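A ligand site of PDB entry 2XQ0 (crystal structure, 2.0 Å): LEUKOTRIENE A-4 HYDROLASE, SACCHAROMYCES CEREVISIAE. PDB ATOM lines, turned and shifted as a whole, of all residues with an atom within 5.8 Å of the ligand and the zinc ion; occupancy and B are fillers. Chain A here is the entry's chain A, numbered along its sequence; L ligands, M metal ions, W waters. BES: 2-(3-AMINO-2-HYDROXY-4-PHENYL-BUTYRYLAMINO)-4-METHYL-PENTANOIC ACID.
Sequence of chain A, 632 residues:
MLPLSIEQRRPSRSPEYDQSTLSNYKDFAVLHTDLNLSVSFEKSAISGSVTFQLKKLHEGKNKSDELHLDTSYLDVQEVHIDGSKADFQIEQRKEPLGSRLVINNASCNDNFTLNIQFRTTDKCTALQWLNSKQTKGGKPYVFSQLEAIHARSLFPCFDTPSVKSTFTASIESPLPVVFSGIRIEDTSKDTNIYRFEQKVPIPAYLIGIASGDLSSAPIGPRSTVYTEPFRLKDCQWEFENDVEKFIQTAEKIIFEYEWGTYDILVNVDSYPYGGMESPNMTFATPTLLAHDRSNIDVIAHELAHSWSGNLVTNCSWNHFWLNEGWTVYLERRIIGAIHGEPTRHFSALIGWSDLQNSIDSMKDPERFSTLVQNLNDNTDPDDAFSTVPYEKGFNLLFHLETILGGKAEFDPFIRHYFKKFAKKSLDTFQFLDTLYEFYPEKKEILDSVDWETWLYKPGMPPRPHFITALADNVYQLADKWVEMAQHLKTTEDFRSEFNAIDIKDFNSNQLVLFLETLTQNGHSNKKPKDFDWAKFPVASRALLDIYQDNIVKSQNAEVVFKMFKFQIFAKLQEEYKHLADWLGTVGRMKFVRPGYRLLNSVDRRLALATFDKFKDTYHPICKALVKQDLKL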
ATOM      1  N   GLN A 145     -39.455 -10.554 -30.980  1.00  0.00           N
ATOM      2  CA  GLN A 145     -38.140 -10.423 -30.381  1.00  0.00           C
ATOM      3  C   GLN A 145     -37.786  -8.952 -30.573  1.00  0.00           C
ATOM      4  O   GLN A 145     -37.558  -8.518 -31.710  1.00  0.00           O
ATOM      5  CB  GLN A 145     -37.129 -11.327 -31.084  1.00  0.00           C
ATOM      6  CG  GLN A 145     -35.673 -10.946 -30.811  1.00  0.00           C
ATOM      7  CD  GLN A 145     -35.328 -11.028 -29.338  1.00  0.00           C
ATOM      8  OE1 GLN A 145     -35.546 -12.067 -28.711  1.00  0.00           O
ATOM      9  NE2 GLN A 145     -34.805  -9.943 -28.786  1.00  0.00           N
ATOM     10  N   GLU A 147     -35.485  -6.890 -28.625  1.00  0.00           N
ATOM     11  CA  GLU A 147     -34.162  -6.342 -28.263  1.00  0.00           C
ATOM     12  C   GLU A 147     -33.283  -6.305 -29.510  1.00  0.00           C
ATOM     13  O   GLU A 147     -33.276  -7.273 -30.262  1.00  0.00           O
ATOM     14  CB  GLU A 147     -33.497  -7.196 -27.183  1.00  0.00           C
ATOM     15  CG  GLU A 147     -32.341  -6.500 -26.448  1.00  0.00           C
ATOM     16  CD  GLU A 147     -31.837  -7.358 -25.292  1.00  0.00           C
ATOM     17  OE1 GLU A 147     -32.431  -8.419 -25.066  1.00  0.00           O
ATOM     18  OE2 GLU A 147     -30.855  -6.989 -24.621  1.00  0.00           O
ATOM     19  N   ALA A 148     -32.562  -5.201 -29.744  1.00  0.00           N
ATOM     20  CA  ALA A 148     -32.497  -4.044 -28.865  1.00  0.00           C
ATOM     21  C   ALA A 148     -33.488  -2.936 -29.226  1.00  0.00           C
ATOM     22  O   ALA A 148     -34.136  -2.383 -28.330  1.00  0.00           O
ATOM     23  CB  ALA A 148     -31.089  -3.469 -28.866  1.00  0.00           C
ATOM     24  N   PRO A 272     -34.343 -17.933 -32.969  1.00  0.00           N
ATOM     25  CA  PRO A 272     -32.929 -17.677 -33.294  1.00  0.00           C
ATOM     26  C   PRO A 272     -31.989 -17.435 -32.107  1.00  0.00           C
ATOM     27  O   PRO A 272     -30.775 -17.437 -32.303  1.00  0.00           O
ATOM     28  CB  PRO A 272     -33.017 -16.400 -34.147  1.00  0.00           C
ATOM     29  CG  PRO A 272     -34.191 -15.666 -33.559  1.00  0.00           C
ATOM     30  CD  PRO A 272     -35.156 -16.704 -33.043  1.00  0.00           C
ATOM     31  N   TYR A 273     -32.513 -17.210 -30.907  1.00  0.00           N
ATOM     32  CA  TYR A 273     -31.661 -17.000 -29.747  1.00  0.00           C
ATOM     33  C   TYR A 273     -31.784 -18.188 -28.817  1.00  0.00           C
ATOM     34  O   TYR A 273     -32.595 -19.079 -29.060  1.00  0.00           O
ATOM     35  CB  TYR A 273     -32.000 -15.681 -29.041  1.00  0.00           C
ATOM     36  CG  TYR A 273     -31.840 -14.497 -29.967  1.00  0.00           C
ATOM     37  CD1 TYR A 273     -30.627 -13.836 -30.075  1.00  0.00           C
ATOM     38  CD2 TYR A 273     -32.894 -14.068 -30.763  1.00  0.00           C
ATOM     39  CE1 TYR A 273     -30.477 -12.759 -30.930  1.00  0.00           C
ATOM     40  CE2 TYR A 273     -32.748 -13.000 -31.619  1.00  0.00           C
ATOM     41  CZ  TYR A 273     -31.544 -12.349 -31.706  1.00  0.00           C
ATOM     42  OH  TYR A 273     -31.397 -11.280 -32.563  1.00  0.00           O
ATOM     43  N   GLY A 274     -30.953 -18.216 -27.782  1.00  0.00           N
ATOM     44  CA  GLY A 274     -30.993 -19.297 -26.817  1.00  0.00           C
ATOM     45  C   GLY A 274     -32.161 -18.979 -25.901  1.00  0.00           C
ATOM     46  O   GLY A 274     -32.891 -19.859 -25.471  1.00  0.00           O
ATOM     47  N   GLY A 275     -32.367 -17.697 -25.635  1.00  0.00           N
ATOM     48  CA  GLY A 275     -33.444 -17.280 -24.756  1.00  0.00           C
ATOM     49  C   GLY A 275     -33.618 -15.788 -24.780  1.00  0.00           C
ATOM     50  O   GLY A 275     -32.748 -15.079 -25.263  1.00  0.00           O
ATOM     51  N   MET A 276     -34.748 -15.308 -24.257  1.00  0.00           N
ATOM     52  CA  MET A 276     -34.991 -13.864 -24.154  1.00  0.00           C
ATOM     53  C   MET A 276     -35.748 -13.703 -22.860  1.00  0.00           C
ATOM     54  O   MET A 276     -36.761 -14.365 -22.645  1.00  0.00           O
ATOM     55  CB  MET A 276     -35.821 -13.329 -25.304  1.00  0.00           C
ATOM     56  CG  MET A 276     -36.204 -11.860 -25.181  1.00  0.00           C
ATOM     57  SD  MET A 276     -34.781 -10.739 -25.025  1.00  0.00           S
ATOM     58  CE  MET A 276     -35.485  -9.398 -24.049  1.00  0.00           C
ATOM     59  N   GLU A 277     -35.247 -12.799 -22.016  1.00  0.00           N
ATOM     60  CA  GLU A 277     -35.719 -12.625 -20.652  1.00  0.00           C
ATOM     61  C   GLU A 277     -36.955 -11.732 -20.504  1.00  0.00           C
ATOM     62  O   GLU A 277     -37.005 -10.898 -19.598  1.00  0.00           O
ATOM     63  CB  GLU A 277     -34.569 -12.006 -19.839  1.00  0.00           C
ATOM     64  CG  GLU A 277     -34.227 -10.519 -20.206  1.00  0.00           C
ATOM     65  CD  GLU A 277     -33.127 -10.368 -21.288  1.00  0.00           C
ATOM     66  OE1 GLU A 277     -32.861 -11.318 -22.062  1.00  0.00           O
ATOM     67  OE2 GLU A 277     -32.518  -9.269 -21.363  1.00  0.00           O
ATOM     68  N   ASP A 297     -28.658 -24.177 -17.931  1.00  0.00           N
ATOM     69  CA  ASP A 297     -28.032 -22.976 -17.423  1.00  0.00           C
ATOM     70  C   ASP A 297     -28.528 -21.764 -18.225  1.00  0.00           C
ATOM     71  O   ASP A 297     -28.582 -20.646 -17.721  1.00  0.00           O
ATOM     72  CB  ASP A 297     -26.524 -23.131 -17.478  1.00  0.00           C
ATOM     73  CG  ASP A 297     -26.064 -24.472 -16.920  1.00  0.00           C
ATOM     74  OD1 ASP A 297     -26.888 -25.146 -16.244  1.00  0.00           O
ATOM     75  OD2 ASP A 297     -24.903 -24.865 -17.167  1.00  0.00           O
ATOM     76  N   VAL A 298     -28.930 -21.996 -19.472  1.00  0.00           N
ATOM     77  CA  VAL A 298     -29.537 -20.917 -20.245  1.00  0.00           C
ATOM     78  C   VAL A 298     -30.736 -20.378 -19.474  1.00  0.00           C
ATOM     79  O   VAL A 298     -31.111 -19.209 -19.637  1.00  0.00           O
ATOM     80  CB  VAL A 298     -30.001 -21.372 -21.643  1.00  0.00           C
ATOM     81  CG1 VAL A 298     -30.747 -20.229 -22.350  1.00  0.00           C
ATOM     82  CG2 VAL A 298     -28.808 -21.853 -22.474  1.00  0.00           C
ATOM     83  N   HIS A 301     -29.425 -18.136 -16.718  1.00  0.00           N
ATOM     84  CA  HIS A 301     -29.147 -16.871 -17.386  1.00  0.00           C
ATOM     85  C   HIS A 301     -30.381 -15.974 -17.478  1.00  0.00           C
ATOM     86  O   HIS A 301     -30.381 -14.875 -16.965  1.00  0.00           O
ATOM     87  CB  HIS A 301     -28.550 -17.087 -18.779  1.00  0.00           C
ATOM     88  CG  HIS A 301     -28.064 -15.813 -19.402  1.00  0.00           C
ATOM     89  ND1 HIS A 301     -26.780 -15.343 -19.244  1.00  0.00           N
ATOM     90  CD2 HIS A 301     -28.716 -14.890 -20.151  1.00  0.00           C
ATOM     91  CE1 HIS A 301     -26.650 -14.189 -19.880  1.00  0.00           C
ATOM     92  NE2 HIS A 301     -27.816 -13.887 -20.434  1.00  0.00           N
ATOM     93  N   GLU A 302     -31.441 -16.443 -18.141  1.00  0.00           N
ATOM     94  CA  GLU A 302     -32.639 -15.629 -18.277  1.00  0.00           C
ATOM     95  C   GLU A 302     -33.222 -15.299 -16.911  1.00  0.00           C
ATOM     96  O   GLU A 302     -33.788 -14.228 -16.707  1.00  0.00           O
ATOM     97  CB  GLU A 302     -33.717 -16.368 -19.081  1.00  0.00           C
ATOM     98  CG  GLU A 302     -33.239 -16.972 -20.395  1.00  0.00           C
ATOM     99  CD  GLU A 302     -32.634 -15.952 -21.313  1.00  0.00           C
ATOM    100  OE1 GLU A 302     -31.885 -16.358 -22.236  1.00  0.00           O
ATOM    101  OE2 GLU A 302     -32.875 -14.738 -21.115  1.00  0.00           O
ATOM    102  N   HIS A 305     -31.523 -12.308 -15.280  1.00  0.00           N
ATOM    103  CA  HIS A 305     -31.984 -11.069 -15.896  1.00  0.00           C
ATOM    104  C   HIS A 305     -33.123 -10.423 -15.111  1.00  0.00           C
ATOM    105  O   HIS A 305     -33.304  -9.194 -15.120  1.00  0.00           O
ATOM    106  CB  HIS A 305     -32.445 -11.309 -17.341  1.00  0.00           C
ATOM    107  CG  HIS A 305     -31.369 -11.132 -18.356  1.00  0.00           C
ATOM    108  ND1 HIS A 305     -30.610  -9.989 -18.432  1.00  0.00           N
ATOM    109  CD2 HIS A 305     -30.931 -11.957 -19.345  1.00  0.00           C
ATOM    110  CE1 HIS A 305     -29.734 -10.118 -19.415  1.00  0.00           C
ATOM    111  NE2 HIS A 305     -29.909 -11.301 -19.980  1.00  0.00           N
ATOM    112  N   PHE A 320     -24.490  -1.480 -22.240  1.00  0.00           N
ATOM    113  CA  PHE A 320     -25.098  -2.812 -22.327  1.00  0.00           C
ATOM    114  C   PHE A 320     -24.423  -3.810 -21.379  1.00  0.00           C
ATOM    115  O   PHE A 320     -25.051  -4.768 -20.938  1.00  0.00           O
ATOM    116  CB  PHE A 320     -25.006  -3.296 -23.774  1.00  0.00           C
ATOM    117  CG  PHE A 320     -25.741  -4.571 -24.051  1.00  0.00           C
ATOM    118  CD1 PHE A 320     -27.066  -4.737 -23.629  1.00  0.00           C
ATOM    119  CD2 PHE A 320     -25.146  -5.594 -24.791  1.00  0.00           C
ATOM    120  CE1 PHE A 320     -27.759  -5.910 -23.906  1.00  0.00           C
ATOM    121  CE2 PHE A 320     -25.826  -6.772 -25.069  1.00  0.00           C
ATOM    122  CZ  PHE A 320     -27.150  -6.918 -24.625  1.00  0.00           C
ATOM    123  N   GLU A 324     -25.768  -7.419 -19.487  1.00  0.00           N
ATOM    124  CA  GLU A 324     -25.238  -8.757 -19.782  1.00  0.00           C
ATOM    125  C   GLU A 324     -24.061  -9.191 -18.905  1.00  0.00           C
ATOM    126  O   GLU A 324     -23.918 -10.363 -18.607  1.00  0.00           O
ATOM    127  CB  GLU A 324     -24.888  -8.893 -21.260  1.00  0.00           C
ATOM    128  CG  GLU A 324     -26.094  -8.773 -22.211  1.00  0.00           C
ATOM    129  CD  GLU A 324     -27.155  -9.843 -21.985  1.00  0.00           C
ATOM    130  OE1 GLU A 324     -26.875 -10.875 -21.331  1.00  0.00           O
ATOM    131  OE2 GLU A 324     -28.291  -9.662 -22.486  1.00  0.00           O
ATOM    132  N   THR A 327     -25.546 -10.149 -15.568  1.00  0.00           N
ATOM    133  CA  THR A 327     -26.278 -11.411 -15.752  1.00  0.00           C
ATOM    134  C   THR A 327     -25.345 -12.619 -15.794  1.00  0.00           C
ATOM    135  O   THR A 327     -25.606 -13.614 -15.134  1.00  0.00           O
ATOM    136  CB  THR A 327     -27.173 -11.377 -17.004  1.00  0.00           C
ATOM    137  OG1 THR A 327     -28.114 -10.300 -16.858  1.00  0.00           O
ATOM    138  CG2 THR A 327     -27.931 -12.714 -17.192  1.00  0.00           C
ATOM    139  N   VAL A 328     -24.271 -12.533 -16.576  1.00  0.00           N
ATOM    140  CA  VAL A 328     -23.338 -13.641 -16.695  1.00  0.00           C
ATOM    141  C   VAL A 328     -22.698 -13.891 -15.332  1.00  0.00           C
ATOM    142  O   VAL A 328     -22.511 -15.044 -14.919  1.00  0.00           O
ATOM    143  CB  VAL A 328     -22.250 -13.388 -17.812  1.00  0.00           C
ATOM    144  CG1 VAL A 328     -21.193 -14.504 -17.809  1.00  0.00           C
ATOM    145  CG2 VAL A 328     -22.900 -13.290 -19.216  1.00  0.00           C
ATOM    146  N   GLU A 331     -25.516 -15.470 -13.100  1.00  0.00           N
ATOM    147  CA  GLU A 331     -25.737 -16.821 -13.613  1.00  0.00           C
ATOM    148  C   GLU A 331     -24.681 -17.774 -13.057  1.00  0.00           C
ATOM    149  O   GLU A 331     -24.993 -18.845 -12.558  1.00  0.00           O
ATOM    150  CB  GLU A 331     -25.624 -16.786 -15.147  1.00  0.00           C
ATOM    151  CG  GLU A 331     -25.602 -18.133 -15.866  1.00  0.00           C
ATOM    152  CD  GLU A 331     -25.218 -17.993 -17.351  1.00  0.00           C
ATOM    153  OE1 GLU A 331     -24.989 -16.842 -17.820  1.00  0.00           O
ATOM    154  OE2 GLU A 331     -25.135 -19.035 -18.033  1.00  0.00           O
ATOM    155  N   ASP A 382     -27.021  -3.251 -32.831  1.00  0.00           N
ATOM    156  CA  ASP A 382     -26.622  -4.618 -33.138  1.00  0.00           C
ATOM    157  C   ASP A 382     -25.120  -4.698 -33.337  1.00  0.00           C
ATOM    158  O   ASP A 382     -24.469  -5.604 -32.821  1.00  0.00           O
ATOM    159  CB  ASP A 382     -27.302  -5.111 -34.433  1.00  0.00           C
ATOM    160  CG  ASP A 382     -28.685  -5.701 -34.193  1.00  0.00           C
ATOM    161  OD1 ASP A 382     -28.973  -6.156 -33.063  1.00  0.00           O
ATOM    162  OD2 ASP A 382     -29.496  -5.716 -35.146  1.00  0.00           O
ATOM    163  N   PHE A 385     -23.116  -5.601 -30.388  1.00  0.00           N
ATOM    164  CA  PHE A 385     -23.344  -6.805 -29.611  1.00  0.00           C
ATOM    165  C   PHE A 385     -22.329  -7.857 -30.035  1.00  0.00           C
ATOM    166  O   PHE A 385     -22.124  -8.143 -31.214  1.00  0.00           O
ATOM    167  CB  PHE A 385     -24.797  -7.294 -29.723  1.00  0.00           C
ATOM    168  CG  PHE A 385     -25.807  -6.279 -29.246  1.00  0.00           C
ATOM    169  CD1 PHE A 385     -25.521  -5.456 -28.167  1.00  0.00           C
ATOM    170  CD2 PHE A 385     -27.020  -6.124 -29.903  1.00  0.00           C
ATOM    171  CE1 PHE A 385     -26.445  -4.510 -27.734  1.00  0.00           C
ATOM    172  CE2 PHE A 385     -27.937  -5.181 -29.463  1.00  0.00           C
ATOM    173  CZ  PHE A 385     -27.652  -4.378 -28.393  1.00  0.00           C
ATOM    174  N   TYR A 390     -20.717  -9.419 -22.321  1.00  0.00           N
ATOM    175  CA  TYR A 390     -20.961 -10.589 -21.498  1.00  0.00           C
ATOM    176  C   TYR A 390     -19.726 -10.934 -20.673  1.00  0.00           C
ATOM    177  O   TYR A 390     -19.762 -10.973 -19.447  1.00  0.00           O
ATOM    178  CB  TYR A 390     -21.319 -11.793 -22.392  1.00  0.00           C
ATOM    179  CG  TYR A 390     -22.648 -11.656 -23.118  1.00  0.00           C
ATOM    180  CD1 TYR A 390     -22.735 -10.950 -24.321  1.00  0.00           C
ATOM    181  CD2 TYR A 390     -23.793 -12.251 -22.616  1.00  0.00           C
ATOM    182  CE1 TYR A 390     -23.966 -10.820 -24.987  1.00  0.00           C
ATOM    183  CE2 TYR A 390     -25.016 -12.123 -23.275  1.00  0.00           C
ATOM    184  CZ  TYR A 390     -25.099 -11.410 -24.450  1.00  0.00           C
ATOM    185  OH  TYR A 390     -26.315 -11.307 -25.097  1.00  0.00           O
ATOM    186  N   ARG A 588     -31.683 -21.902 -34.335  1.00  0.00           N
ATOM    187  CA  ARG A 588     -30.852 -21.117 -33.419  1.00  0.00           C
ATOM    188  C   ARG A 588     -29.586 -20.615 -34.117  1.00  0.00           C
ATOM    189  O   ARG A 588     -28.796 -21.415 -34.605  1.00  0.00           O
ATOM    190  CB  ARG A 588     -30.486 -21.954 -32.185  1.00  0.00           C
ATOM    191  CG  ARG A 588     -29.769 -21.162 -31.102  1.00  0.00           C
ATOM    192  CD  ARG A 588     -29.652 -21.969 -29.822  1.00  0.00           C
ATOM    193  NE  ARG A 588     -28.943 -21.235 -28.786  1.00  0.00           N
ATOM    194  CZ  ARG A 588     -28.553 -21.745 -27.634  1.00  0.00           C
ATOM    195  NH1 ARG A 588     -28.816 -23.010 -27.343  1.00  0.00           N
ATOM    196  NH2 ARG A 588     -27.900 -20.991 -26.757  1.00  0.00           N
HETATM  197  N2  BES L   1     -31.788 -11.142 -24.596  1.00  0.00           N
HETATM  198  C1  BES L   1     -30.500 -11.799 -24.727  1.00  0.00           C
HETATM  199  C6  BES L   1     -30.217 -12.135 -26.190  1.00  0.00           C
HETATM  200  C7  BES L   1     -30.118 -10.863 -27.000  1.00  0.00           C
HETATM  201  C8  BES L   1     -29.354  -9.801 -26.543  1.00  0.00           C
HETATM  202  C12 BES L   1     -30.811 -10.754 -28.203  1.00  0.00           C
HETATM  203  C9  BES L   1     -29.262  -8.627 -27.282  1.00  0.00           C
HETATM  204  C11 BES L   1     -30.726  -9.577 -28.949  1.00  0.00           C
HETATM  205  C10 BES L   1     -29.949  -8.519 -28.493  1.00  0.00           C
HETATM  206  C2  BES L   1     -30.431 -13.069 -23.866  1.00  0.00           C
HETATM  207  O2  BES L   1     -30.705 -12.869 -22.471  1.00  0.00           O
HETATM  208  C3  BES L   1     -29.062 -13.635 -24.028  1.00  0.00           C
HETATM  209  O3  BES L   1     -28.081 -13.108 -23.514  1.00  0.00           O
HETATM  210  N1  BES L   1     -29.105 -14.723 -24.795  1.00  0.00           N
HETATM  211  C4  BES L   1     -28.005 -15.572 -25.205  1.00  0.00           C
HETATM  212  C13 BES L   1     -28.049 -16.717 -24.202  1.00  0.00           C
HETATM  213  C14 BES L   1     -26.713 -16.960 -23.514  1.00  0.00           C
HETATM  214  C15 BES L   1     -26.932 -17.705 -22.204  1.00  0.00           C
HETATM  215  C16 BES L   1     -25.943 -15.662 -23.279  1.00  0.00           C
HETATM  216  C5  BES L   1     -28.346 -16.092 -26.563  1.00  0.00           C
HETATM  217  O1  BES L   1     -27.430 -16.428 -27.344  1.00  0.00           O
HETATM  218  O4  BES L   1     -29.566 -16.170 -26.876  1.00  0.00           O
HETATM  219 ZN    ZN M   1     -28.725 -12.139 -21.421  1.00  0.00          ZN
HETATM  220  O   HOH W   1     -28.059 -18.810 -28.550  1.00  0.00           O
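N2 of the ligand is in salt-bridge range of OE1 of Glu 277, 2.8 Å away.
The backbone NH of Gly 274 lies within hydrogen-bond range of an oxygen (O4) of the ligand (2.6 Å).
The backbone NH of Gly 275 is in hydrogen-bond range of an oxygen (O4) of the ligand (3.4 Å).
The side-chain carboxylate (OE2) of Glu 302 lies close to an oxygen (O2) of the ligand, at 3.2 Å.
An oxygen (O3) of the ligand lies close to the side-chain hydroxyl (OH) of Tyr 390, 3.0 Å away.
SD of Met 276 sits at hydrogen-bond distance from N2 of the ligand (3.1 Å).
A nitrogen (N2) of the ligand lies within salt-bridge range of the side-chain carboxylate (OE1) of Glu 147.
N of Glu 147 sits close to NE2 of Gln 145 (3.1 Å).
A ring nitrogen (ND1) of His 305 lies within hydrogen-bond range of the side-chain hydroxyl of Thr 327.
The side-chain carboxylate of Glu 331 sits at hydrogen-bond distance from a ring nitrogen (ND1) of His 301, 2.7 Å away.
The backbone NH of Glu 277 is in hydrogen-bond range of the side-chain carboxylate of Glu 302, 3.2 Å away.
Residues that only touch the ligand: Tyr 273 (3.3 Å) and Phe 320 (3.8 Å).
Hydrophobic or aromatic side chains within 4 Å of the ligand: Tyr 273, Met 276, His 301, His 305, Phe 320 and Tyr 390.
12 residues have an atom within 4 Å of the ligand: Glu 147, Tyr 273, Gly 274, Gly 275, Met 276, Glu 277, His 301, Glu 302, His 305, Phe 320, Glu 324 and Tyr 390.
The zinc ion is bound by a ring nitrogen (NE2) of His 305 (2.0 Å), a ring nitrogen (NE2) of His 301 (2.2 Å), the side-chain carboxylate (OE1) of Glu 324 (2.2 Å), an oxygen (O2) of the ligand (2.4 Å) and an oxygen (O3) of the ligand (2.4 Å).
Slightly farther from the zinc ion lies the side-chain carboxylate (OE2) of Glu 324 (2.7 Å).
Water W1 lies within hydrogen-bond range of NE of Arg 588 (2.6 Å), O1 of the ligand (2.7 Å) and N of Gly 274 (3.1 Å).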
